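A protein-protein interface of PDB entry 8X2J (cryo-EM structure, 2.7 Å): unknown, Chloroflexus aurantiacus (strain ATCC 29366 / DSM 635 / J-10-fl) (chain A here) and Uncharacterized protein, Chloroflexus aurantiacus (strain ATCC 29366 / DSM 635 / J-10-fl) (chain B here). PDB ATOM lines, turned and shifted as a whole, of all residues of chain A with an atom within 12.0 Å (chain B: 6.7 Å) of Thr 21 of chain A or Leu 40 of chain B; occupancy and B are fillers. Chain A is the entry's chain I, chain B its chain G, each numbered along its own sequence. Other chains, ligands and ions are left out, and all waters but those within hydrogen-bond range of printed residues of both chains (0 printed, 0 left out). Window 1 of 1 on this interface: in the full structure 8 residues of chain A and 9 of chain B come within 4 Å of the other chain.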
ATOM      1  N   VAL A  11       8.263  12.760 -11.591  1.00  0.00           N
ATOM      2  CA  VAL A  11       7.614  12.592 -12.891  1.00  0.00           C
ATOM      3  C   VAL A  11       8.347  11.558 -13.737  1.00  0.00           C
ATOM      4  O   VAL A  11       7.728  10.660 -14.321  1.00  0.00           O
ATOM      5  CB  VAL A  11       7.513  13.952 -13.604  1.00  0.00           C
ATOM      6  CG1 VAL A  11       7.304  13.790 -15.106  1.00  0.00           C
ATOM      7  CG2 VAL A  11       6.386  14.739 -13.007  1.00  0.00           C
ATOM      8  N   LYS A  12       9.667  11.648 -13.804  1.00  0.00           N
ATOM      9  CA  LYS A  12      10.393  10.657 -14.590  1.00  0.00           C
ATOM     10  C   LYS A  12      10.476   9.295 -13.887  1.00  0.00           C
ATOM     11  O   LYS A  12      10.412   8.280 -14.592  1.00  0.00           O
ATOM     12  CB  LYS A  12      11.780  11.188 -14.984  1.00  0.00           C
ATOM     13  CG  LYS A  12      11.742  12.249 -16.071  1.00  0.00           C
ATOM     14  CD  LYS A  12      13.097  12.431 -16.735  1.00  0.00           C
ATOM     15  CE  LYS A  12      13.028  13.476 -17.839  1.00  0.00           C
ATOM     16  NZ  LYS A  12      14.305  13.574 -18.598  1.00  0.00           N
ATOM     17  N   PRO A  13      10.612   9.193 -12.542  1.00  0.00           N
ATOM     18  CA  PRO A  13      10.374   7.877 -11.910  1.00  0.00           C
ATOM     19  C   PRO A  13       8.999   7.277 -12.167  1.00  0.00           C
ATOM     20  O   PRO A  13       8.912   6.066 -12.405  1.00  0.00           O
ATOM     21  CB  PRO A  13      10.578   8.154 -10.413  1.00  0.00           C
ATOM     22  CG  PRO A  13      11.232   9.453 -10.304  1.00  0.00           C
ATOM     23  CD  PRO A  13      11.462  10.018 -11.657  1.00  0.00           C
ATOM     24  N   VAL A  14       7.926   8.072 -12.166  1.00  0.00           N
ATOM     25  CA  VAL A  14       6.620   7.455 -12.386  1.00  0.00           C
ATOM     26  C   VAL A  14       6.412   7.138 -13.870  1.00  0.00           C
ATOM     27  O   VAL A  14       5.723   6.168 -14.201  1.00  0.00           O
ATOM     28  CB  VAL A  14       5.481   8.315 -11.790  1.00  0.00           C
ATOM     29  CG1 VAL A  14       5.172   9.546 -12.622  1.00  0.00           C
ATOM     30  CG2 VAL A  14       4.225   7.484 -11.581  1.00  0.00           C
ATOM     31  N   PHE A  15       7.049   7.885 -14.783  1.00  0.00           N
ATOM     32  CA  PHE A  15       6.987   7.527 -16.198  1.00  0.00           C
ATOM     33  C   PHE A  15       7.761   6.248 -16.485  1.00  0.00           C
ATOM     34  O   PHE A  15       7.292   5.397 -17.251  1.00  0.00           O
ATOM     35  CB  PHE A  15       7.509   8.673 -17.067  1.00  0.00           C
ATOM     36  CG  PHE A  15       6.514   9.782 -17.286  1.00  0.00           C
ATOM     37  CD1 PHE A  15       5.185   9.632 -16.920  1.00  0.00           C
ATOM     38  CD2 PHE A  15       6.910  10.973 -17.878  1.00  0.00           C
ATOM     39  CE1 PHE A  15       4.272  10.651 -17.131  1.00  0.00           C
ATOM     40  CE2 PHE A  15       6.003  11.996 -18.090  1.00  0.00           C
ATOM     41  CZ  PHE A  15       4.682  11.833 -17.717  1.00  0.00           C
ATOM     42  N   LEU A  16       8.942   6.088 -15.876  1.00  0.00           N
ATOM     43  CA  LEU A  16       9.662   4.822 -15.996  1.00  0.00           C
ATOM     44  C   LEU A  16       8.916   3.670 -15.334  1.00  0.00           C
ATOM     45  O   LEU A  16       8.965   2.548 -15.842  1.00  0.00           O
ATOM     46  CB  LEU A  16      11.084   4.938 -15.438  1.00  0.00           C
ATOM     47  CG  LEU A  16      12.232   5.414 -16.348  1.00  0.00           C
ATOM     48  CD1 LEU A  16      12.438   4.391 -17.454  1.00  0.00           C
ATOM     49  CD2 LEU A  16      12.049   6.792 -16.964  1.00  0.00           C
ATOM     50  N   ALA A  17       8.193   3.926 -14.238  1.00  0.00           N
ATOM     51  CA  ALA A  17       7.382   2.876 -13.621  1.00  0.00           C
ATOM     52  C   ALA A  17       6.221   2.452 -14.520  1.00  0.00           C
ATOM     53  O   ALA A  17       5.952   1.253 -14.663  1.00  0.00           O
ATOM     54  CB  ALA A  17       6.864   3.341 -12.262  1.00  0.00           C
ATOM     55  N   VAL A  18       5.538   3.418 -15.145  1.00  0.00           N
ATOM     56  CA  VAL A  18       4.430   3.102 -16.049  1.00  0.00           C
ATOM     57  C   VAL A  18       4.927   2.374 -17.296  1.00  0.00           C
ATOM     58  O   VAL A  18       4.327   1.377 -17.721  1.00  0.00           O
ATOM     59  CB  VAL A  18       3.644   4.382 -16.396  1.00  0.00           C
ATOM     60  CG1 VAL A  18       2.635   4.127 -17.500  1.00  0.00           C
ATOM     61  CG2 VAL A  18       2.898   4.879 -15.173  1.00  0.00           C
ATOM     62  N   THR A  19       6.041   2.828 -17.883  1.00  0.00           N
ATOM     63  CA  THR A  19       6.566   2.154 -19.070  1.00  0.00           C
ATOM     64  C   THR A  19       7.134   0.777 -18.742  1.00  0.00           C
ATOM     65  O   THR A  19       7.014  -0.144 -19.559  1.00  0.00           O
ATOM     66  CB  THR A  19       7.633   3.009 -19.753  1.00  0.00           C
ATOM     67  OG1 THR A  19       8.628   3.393 -18.798  1.00  0.00           O
ATOM     68  CG2 THR A  19       7.007   4.253 -20.367  1.00  0.00           C
ATOM     69  N   LEU A  20       7.737   0.611 -17.559  1.00  0.00           N
ATOM     70  CA  LEU A  20       8.213  -0.699 -17.132  1.00  0.00           C
ATOM     71  C   LEU A  20       7.056  -1.658 -16.902  1.00  0.00           C
ATOM     72  O   LEU A  20       7.138  -2.831 -17.283  1.00  0.00           O
ATOM     73  CB  LEU A  20       9.055  -0.560 -15.865  1.00  0.00           C
ATOM     74  CG  LEU A  20       9.980  -1.725 -15.518  1.00  0.00           C
ATOM     75  CD1 LEU A  20      10.953  -1.988 -16.655  1.00  0.00           C
ATOM     76  CD2 LEU A  20      10.725  -1.443 -14.224  1.00  0.00           C
ATOM     77  N   THR A  21       5.966  -1.172 -16.297  1.00  0.00           N
ATOM     78  CA  THR A  21       4.768  -1.989 -16.126  1.00  0.00           C
ATOM     79  C   THR A  21       4.166  -2.378 -17.470  1.00  0.00           C
ATOM     80  O   THR A  21       3.770  -3.534 -17.668  1.00  0.00           O
ATOM     81  CB  THR A  21       3.740  -1.236 -15.281  1.00  0.00           C
ATOM     82  OG1 THR A  21       4.350  -0.797 -14.062  1.00  0.00           O
ATOM     83  CG2 THR A  21       2.555  -2.129 -14.958  1.00  0.00           C
ATOM     84  N   GLY A  22       4.128  -1.432 -18.411  1.00  0.00           N
ATOM     85  CA  GLY A  22       3.599  -1.721 -19.734  1.00  0.00           C
ATOM     86  C   GLY A  22       4.428  -2.733 -20.502  1.00  0.00           C
ATOM     87  O   GLY A  22       3.879  -3.640 -21.129  1.00  0.00           O
ATOM     88  N   MET A  23       5.760  -2.621 -20.432  1.00  0.00           N
ATOM     89  CA  MET A  23       6.595  -3.568 -21.166  1.00  0.00           C
ATOM     90  C   MET A  23       6.630  -4.939 -20.495  1.00  0.00           C
ATOM     91  O   MET A  23       6.681  -5.956 -21.197  1.00  0.00           O
ATOM     92  CB  MET A  23       8.007  -3.001 -21.369  1.00  0.00           C
ATOM     93  CG  MET A  23       8.871  -2.852 -20.129  1.00  0.00           C
ATOM     94  SD  MET A  23      10.061  -4.194 -19.937  1.00  0.00           S
ATOM     95  CE  MET A  23      11.221  -3.808 -21.246  1.00  0.00           C
ATOM     96  N   VAL A  24       6.556  -5.000 -19.158  1.00  0.00           N
ATOM     97  CA  VAL A  24       6.480  -6.289 -18.471  1.00  0.00           C
ATOM     98  C   VAL A  24       5.156  -6.984 -18.770  1.00  0.00           C
ATOM     99  O   VAL A  24       5.129  -8.184 -19.076  1.00  0.00           O
ATOM    100  CB  VAL A  24       6.711  -6.101 -16.957  1.00  0.00           C
ATOM    101  CG1 VAL A  24       6.265  -7.318 -16.171  1.00  0.00           C
ATOM    102  CG2 VAL A  24       8.187  -5.860 -16.685  1.00  0.00           C
ATOM    103  N   ALA A  25       4.045  -6.236 -18.733  1.00  0.00           N
ATOM    104  CA  ALA A  25       2.743  -6.808 -19.060  1.00  0.00           C
ATOM    105  C   ALA A  25       2.666  -7.228 -20.523  1.00  0.00           C
ATOM    106  O   ALA A  25       2.089  -8.275 -20.836  1.00  0.00           O
ATOM    107  CB  ALA A  25       1.633  -5.814 -18.727  1.00  0.00           C
ATOM    108  N   PHE A  26       3.262  -6.442 -21.427  1.00  0.00           N
ATOM    109  CA  PHE A  26       3.276  -6.794 -22.844  1.00  0.00           C
ATOM    110  C   PHE A  26       4.085  -8.060 -23.096  1.00  0.00           C
ATOM    111  O   PHE A  26       3.631  -8.956 -23.814  1.00  0.00           O
ATOM    112  CB  PHE A  26       3.834  -5.631 -23.667  1.00  0.00           C
ATOM    113  CG  PHE A  26       4.170  -5.999 -25.086  1.00  0.00           C
ATOM    114  CD1 PHE A  26       3.164  -6.254 -26.004  1.00  0.00           C
ATOM    115  CD2 PHE A  26       5.490  -6.092 -25.500  1.00  0.00           C
ATOM    116  CE1 PHE A  26       3.466  -6.594 -27.309  1.00  0.00           C
ATOM    117  CE2 PHE A  26       5.799  -6.434 -26.804  1.00  0.00           C
ATOM    118  CZ  PHE A  26       4.786  -6.684 -27.708  1.00  0.00           C
ATOM    119  N   LEU A  27       5.283  -8.156 -22.502  1.00  0.00           N
ATOM    120  CA  LEU A  27       6.111  -9.347 -22.666  1.00  0.00           C
ATOM    121  C   LEU A  27       5.464 -10.575 -22.044  1.00  0.00           C
ATOM    122  O   LEU A  27       5.576 -11.677 -22.591  1.00  0.00           O
ATOM    123  CB  LEU A  27       7.492  -9.122 -22.052  1.00  0.00           C
ATOM    124  CG  LEU A  27       8.505  -8.350 -22.894  1.00  0.00           C
ATOM    125  CD1 LEU A  27       9.836  -8.263 -22.168  1.00  0.00           C
ATOM    126  CD2 LEU A  27       8.673  -8.999 -24.259  1.00  0.00           C
ATOM    127  N   LEU A  28       4.753 -10.396 -20.933  1.00  0.00           N
ATOM    128  CA  LEU A  28       4.088 -11.514 -20.278  1.00  0.00           C
ATOM    129  C   LEU A  28       2.886 -12.000 -21.085  1.00  0.00           C
ATOM    130  O   LEU A  28       2.656 -13.211 -21.199  1.00  0.00           O
ATOM    131  CB  LEU A  28       3.682 -11.076 -18.876  1.00  0.00           C
ATOM    132  CG  LEU A  28       3.545 -12.080 -17.750  1.00  0.00           C
ATOM    133  CD1 LEU A  28       4.804 -12.907 -17.620  1.00  0.00           C
ATOM    134  CD2 LEU A  28       3.326 -11.271 -16.507  1.00  0.00           C
ATOM    135  N   MET A  29       2.123 -11.068 -21.672  1.00  0.00           N
ATOM    136  CA  MET A  29       1.018 -11.444 -22.551  1.00  0.00           C
ATOM    137  C   MET A  29       1.525 -12.119 -23.821  1.00  0.00           C
ATOM    138  O   MET A  29       0.910 -13.073 -24.309  1.00  0.00           O
ATOM    139  CB  MET A  29       0.179 -10.214 -22.904  1.00  0.00           C
ATOM    140  CG  MET A  29      -0.680  -9.675 -21.770  1.00  0.00           C
ATOM    141  SD  MET A  29      -2.305 -10.431 -21.648  1.00  0.00           S
ATOM    142  CE  MET A  29      -2.067 -11.454 -20.203  1.00  0.00           C
ATOM    143  N   VAL A  30       2.649 -11.634 -24.365  1.00  0.00           N
ATOM    144  CA  VAL A  30       3.264 -12.258 -25.538  1.00  0.00           C
ATOM    145  C   VAL A  30       3.742 -13.668 -25.210  1.00  0.00           C
ATOM    146  O   VAL A  30       3.540 -14.597 -26.000  1.00  0.00           O
ATOM    147  CB  VAL A  30       4.399 -11.363 -26.079  1.00  0.00           C
ATOM    148  CG1 VAL A  30       5.317 -12.120 -27.024  1.00  0.00           C
ATOM    149  CG2 VAL A  30       3.807 -10.189 -26.828  1.00  0.00           C
ATOM    150  N   LEU B  35       5.715   2.754  -4.876  1.00  0.00           N
ATOM    151  CA  LEU B  35       4.568   1.875  -4.684  1.00  0.00           C
ATOM    152  C   LEU B  35       4.118   1.249  -5.999  1.00  0.00           C
ATOM    153  O   LEU B  35       3.657   0.103  -6.005  1.00  0.00           O
ATOM    154  CB  LEU B  35       3.423   2.643  -4.025  1.00  0.00           C
ATOM    155  CG  LEU B  35       3.518   2.708  -2.499  1.00  0.00           C
ATOM    156  CD1 LEU B  35       2.468   3.638  -1.925  1.00  0.00           C
ATOM    157  CD2 LEU B  35       3.400   1.320  -1.890  1.00  0.00           C
ATOM    158  N   MET B  36       4.267   1.973  -7.115  1.00  0.00           N
ATOM    159  CA  MET B  36       4.027   1.388  -8.433  1.00  0.00           C
ATOM    160  C   MET B  36       5.005   0.257  -8.724  1.00  0.00           C
ATOM    161  O   MET B  36       4.616  -0.786  -9.260  1.00  0.00           O
ATOM    162  CB  MET B  36       4.138   2.458  -9.520  1.00  0.00           C
ATOM    163  CG  MET B  36       3.332   3.718  -9.281  1.00  0.00           C
ATOM    164  SD  MET B  36       1.675   3.651  -9.979  1.00  0.00           S
ATOM    165  CE  MET B  36       1.039   5.255  -9.497  1.00  0.00           C
ATOM    166  N   ILE B  37       6.277   0.444  -8.363  1.00  0.00           N
ATOM    167  CA  ILE B  37       7.294  -0.582  -8.582  1.00  0.00           C
ATOM    168  C   ILE B  37       7.029  -1.805  -7.707  1.00  0.00           C
ATOM    169  O   ILE B  37       7.134  -2.948  -8.170  1.00  0.00           O
ATOM    170  CB  ILE B  37       8.695   0.018  -8.344  1.00  0.00           C
ATOM    171  CG1 ILE B  37       9.068   0.950  -9.498  1.00  0.00           C
ATOM    172  CG2 ILE B  37       9.760  -1.058  -8.182  1.00  0.00           C
ATOM    173  CD1 ILE B  37       9.065   0.275 -10.853  1.00  0.00           C
ATOM    174  N   ALA B  38       6.646  -1.586  -6.444  1.00  0.00           N
ATOM    175  CA  ALA B  38       6.333  -2.697  -5.545  1.00  0.00           C
ATOM    176  C   ALA B  38       5.086  -3.453  -5.992  1.00  0.00           C
ATOM    177  O   ALA B  38       5.050  -4.690  -5.931  1.00  0.00           O
ATOM    178  CB  ALA B  38       6.165  -2.183  -4.117  1.00  0.00           C
ATOM    179  N   GLY B  39       4.059  -2.734  -6.454  1.00  0.00           N
ATOM    180  CA  GLY B  39       2.876  -3.396  -6.979  1.00  0.00           C
ATOM    181  C   GLY B  39       3.148  -4.160  -8.260  1.00  0.00           C
ATOM    182  O   GLY B  39       2.589  -5.237  -8.479  1.00  0.00           O
ATOM    183  N   LEU B  40       4.024  -3.623  -9.116  1.00  0.00           N
ATOM    184  CA  LEU B  40       4.431  -4.333 -10.323  1.00  0.00           C
ATOM    185  C   LEU B  40       5.230  -5.588  -9.987  1.00  0.00           C
ATOM    186  O   LEU B  40       5.076  -6.620 -10.648  1.00  0.00           O
ATOM    187  CB  LEU B  40       5.237  -3.400 -11.227  1.00  0.00           C
ATOM    188  CG  LEU B  40       5.965  -3.992 -12.434  1.00  0.00           C
ATOM    189  CD1 LEU B  40       4.976  -4.600 -13.414  1.00  0.00           C
ATOM    190  CD2 LEU B  40       6.824  -2.938 -13.109  1.00  0.00           C
ATOM    191  N   MET B  41       6.079  -5.522  -8.956  1.00  0.00           N
ATOM    192  CA  MET B  41       6.829  -6.700  -8.526  1.00  0.00           C
ATOM    193  C   MET B  41       5.909  -7.770  -7.950  1.00  0.00           C
ATOM    194  O   MET B  41       6.100  -8.964  -8.211  1.00  0.00           O
ATOM    195  CB  MET B  41       7.892  -6.301  -7.502  1.00  0.00           C
ATOM    196  CG  MET B  41       9.116  -5.634  -8.106  1.00  0.00           C
ATOM    197  SD  MET B  41       9.900  -6.635  -9.384  1.00  0.00           S
ATOM    198  CE  MET B  41       9.671  -5.592 -10.823  1.00  0.00           C
ATOM    199  N   VAL B  42       4.900  -7.356  -7.174  1.00  0.00           N
ATOM    200  CA  VAL B  42       3.915  -8.295  -6.635  1.00  0.00           C
ATOM    201  C   VAL B  42       3.108  -8.935  -7.764  1.00  0.00           C
ATOM    202  O   VAL B  42       2.882 -10.154  -7.772  1.00  0.00           O
ATOM    203  CB  VAL B  42       3.014  -7.573  -5.611  1.00  0.00           C
ATOM    204  CG1 VAL B  42       1.738  -8.353  -5.331  1.00  0.00           C
ATOM    205  CG2 VAL B  42       3.779  -7.330  -4.319  1.00  0.00           C
ATOM    206  N   PHE B  43       2.699  -8.127  -8.749  1.00  0.00           N
ATOM    207  CA  PHE B  43       1.954  -8.629  -9.901  1.00  0.00           C
ATOM    208  C   PHE B  43       2.794  -9.592 -10.735  1.00  0.00           C
ATOM    209  O   PHE B  43       2.289 -10.619 -11.201  1.00  0.00           O
ATOM    210  CB  PHE B  43       1.470  -7.440 -10.738  1.00  0.00           C
ATOM    211  CG  PHE B  43       1.301  -7.734 -12.204  1.00  0.00           C
ATOM    212  CD1 PHE B  43       0.200  -8.439 -12.663  1.00  0.00           C
ATOM    213  CD2 PHE B  43       2.225  -7.266 -13.130  1.00  0.00           C
ATOM    214  CE1 PHE B  43       0.036  -8.697 -14.012  1.00  0.00           C
ATOM    215  CE2 PHE B  43       2.067  -7.522 -14.479  1.00  0.00           C
ATOM    216  CZ  PHE B  43       0.971  -8.237 -14.920  1.00  0.00           C
ATOM    217  N   LEU B  44       4.084  -9.289 -10.906  1.00  0.00           N
ATOM    218  CA  LEU B  44       4.979 -10.162 -11.658  1.00  0.00           C
ATOM    219  C   LEU B  44       5.211 -11.486 -10.938  1.00  0.00           C
ATOM    220  O   LEU B  44       5.201 -12.547 -11.574  1.00  0.00           O
ATOM    221  CB  LEU B  44       6.305  -9.446 -11.908  1.00  0.00           C
ATOM    222  CG  LEU B  44       7.432 -10.242 -12.561  1.00  0.00           C
ATOM    223  CD1 LEU B  44       7.246 -10.282 -14.065  1.00  0.00           C
ATOM    224  CD2 LEU B  44       8.781  -9.645 -12.201  1.00  0.00           C
ATOM    225  N   VAL B  45       5.407 -11.444  -9.616  1.00  0.00           N
ATOM    226  CA  VAL B  45       5.613 -12.666  -8.841  1.00  0.00           C
ATOM    227  C   VAL B  45       4.363 -13.540  -8.872  1.00  0.00           C
ATOM    228  O   VAL B  45       4.445 -14.752  -9.116  1.00  0.00           O
ATOM    229  CB  VAL B  45       6.039 -12.309  -7.404  1.00  0.00           C
ATOM    230  CG1 VAL B  45       5.779 -13.459  -6.439  1.00  0.00           C
ATOM    231  CG2 VAL B  45       7.507 -11.915  -7.375  1.00  0.00           C
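O of Ala 17 of chain A is in hydrogen-bond range of OG1 of Thr 21 of chain A (2.7 Å).
Among the printed residues, merely in contact across the chains: Ala 17 of chain A with Met 36 of chain B (3.97 Å), Thr 21 of chain A with Leu 40 of chain B (3.4 Å) and Val 24 of chain A with Leu 44 of chain B (3.8 Å).
Of chain B, only Leu 40 (3.4 Å) comes within 4 Å of Thr 21 of chain A.
Printed residues of chain A within 4 Å of Leu 40 of chain B: Thr 21 (3.4 Å).
No residue of chain A comes within 4 Å of Ile 37 of chain B.
No residue of chain A comes within 4 Å of Ala 38 of chain B.
Gly 39 of chain B touches none of the printed residues of chain A.
Leu 44 of chain B touches just one residue of chain A: Val 24.
Of the printed residues of chain B, Ala 17 of chain A touches Met 36 (3.97 Å).
Of the printed residues of chain B, Val 24 of chain A touches Leu 44 (3.8 Å).
Of the printed residues of chain A, Met 36 of chain B touches Ala 17 (3.97 Å).
Val 14 of chain A touches none of the printed residues of chain B.
The nearest printed residue of chain A that does not touch Leu 40 of chain B is Leu 20 of chain A (4.01 Å).
The nearest printed residue of chain B that does not touch Val 24 of chain A is Leu 40 of chain B (4.1 Å).
Printed residues of chain A that touch a printed residue of chain B: Ala 17, Thr 21 and Val 24.
Hydrophobic or aromatic side chains of chain A that line the printed part of chain B: Ala 17 and Val 24.
Along chain A the printed residues that touch a printed residue of chain B span positions 17 to 24.
Hydrophobic or aromatic side chains of chain B within 4 Å of the printed part of chain A: Met 36, Leu 40 and Leu 44.
Among the printed residues, 3 pairs touch across the chains.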
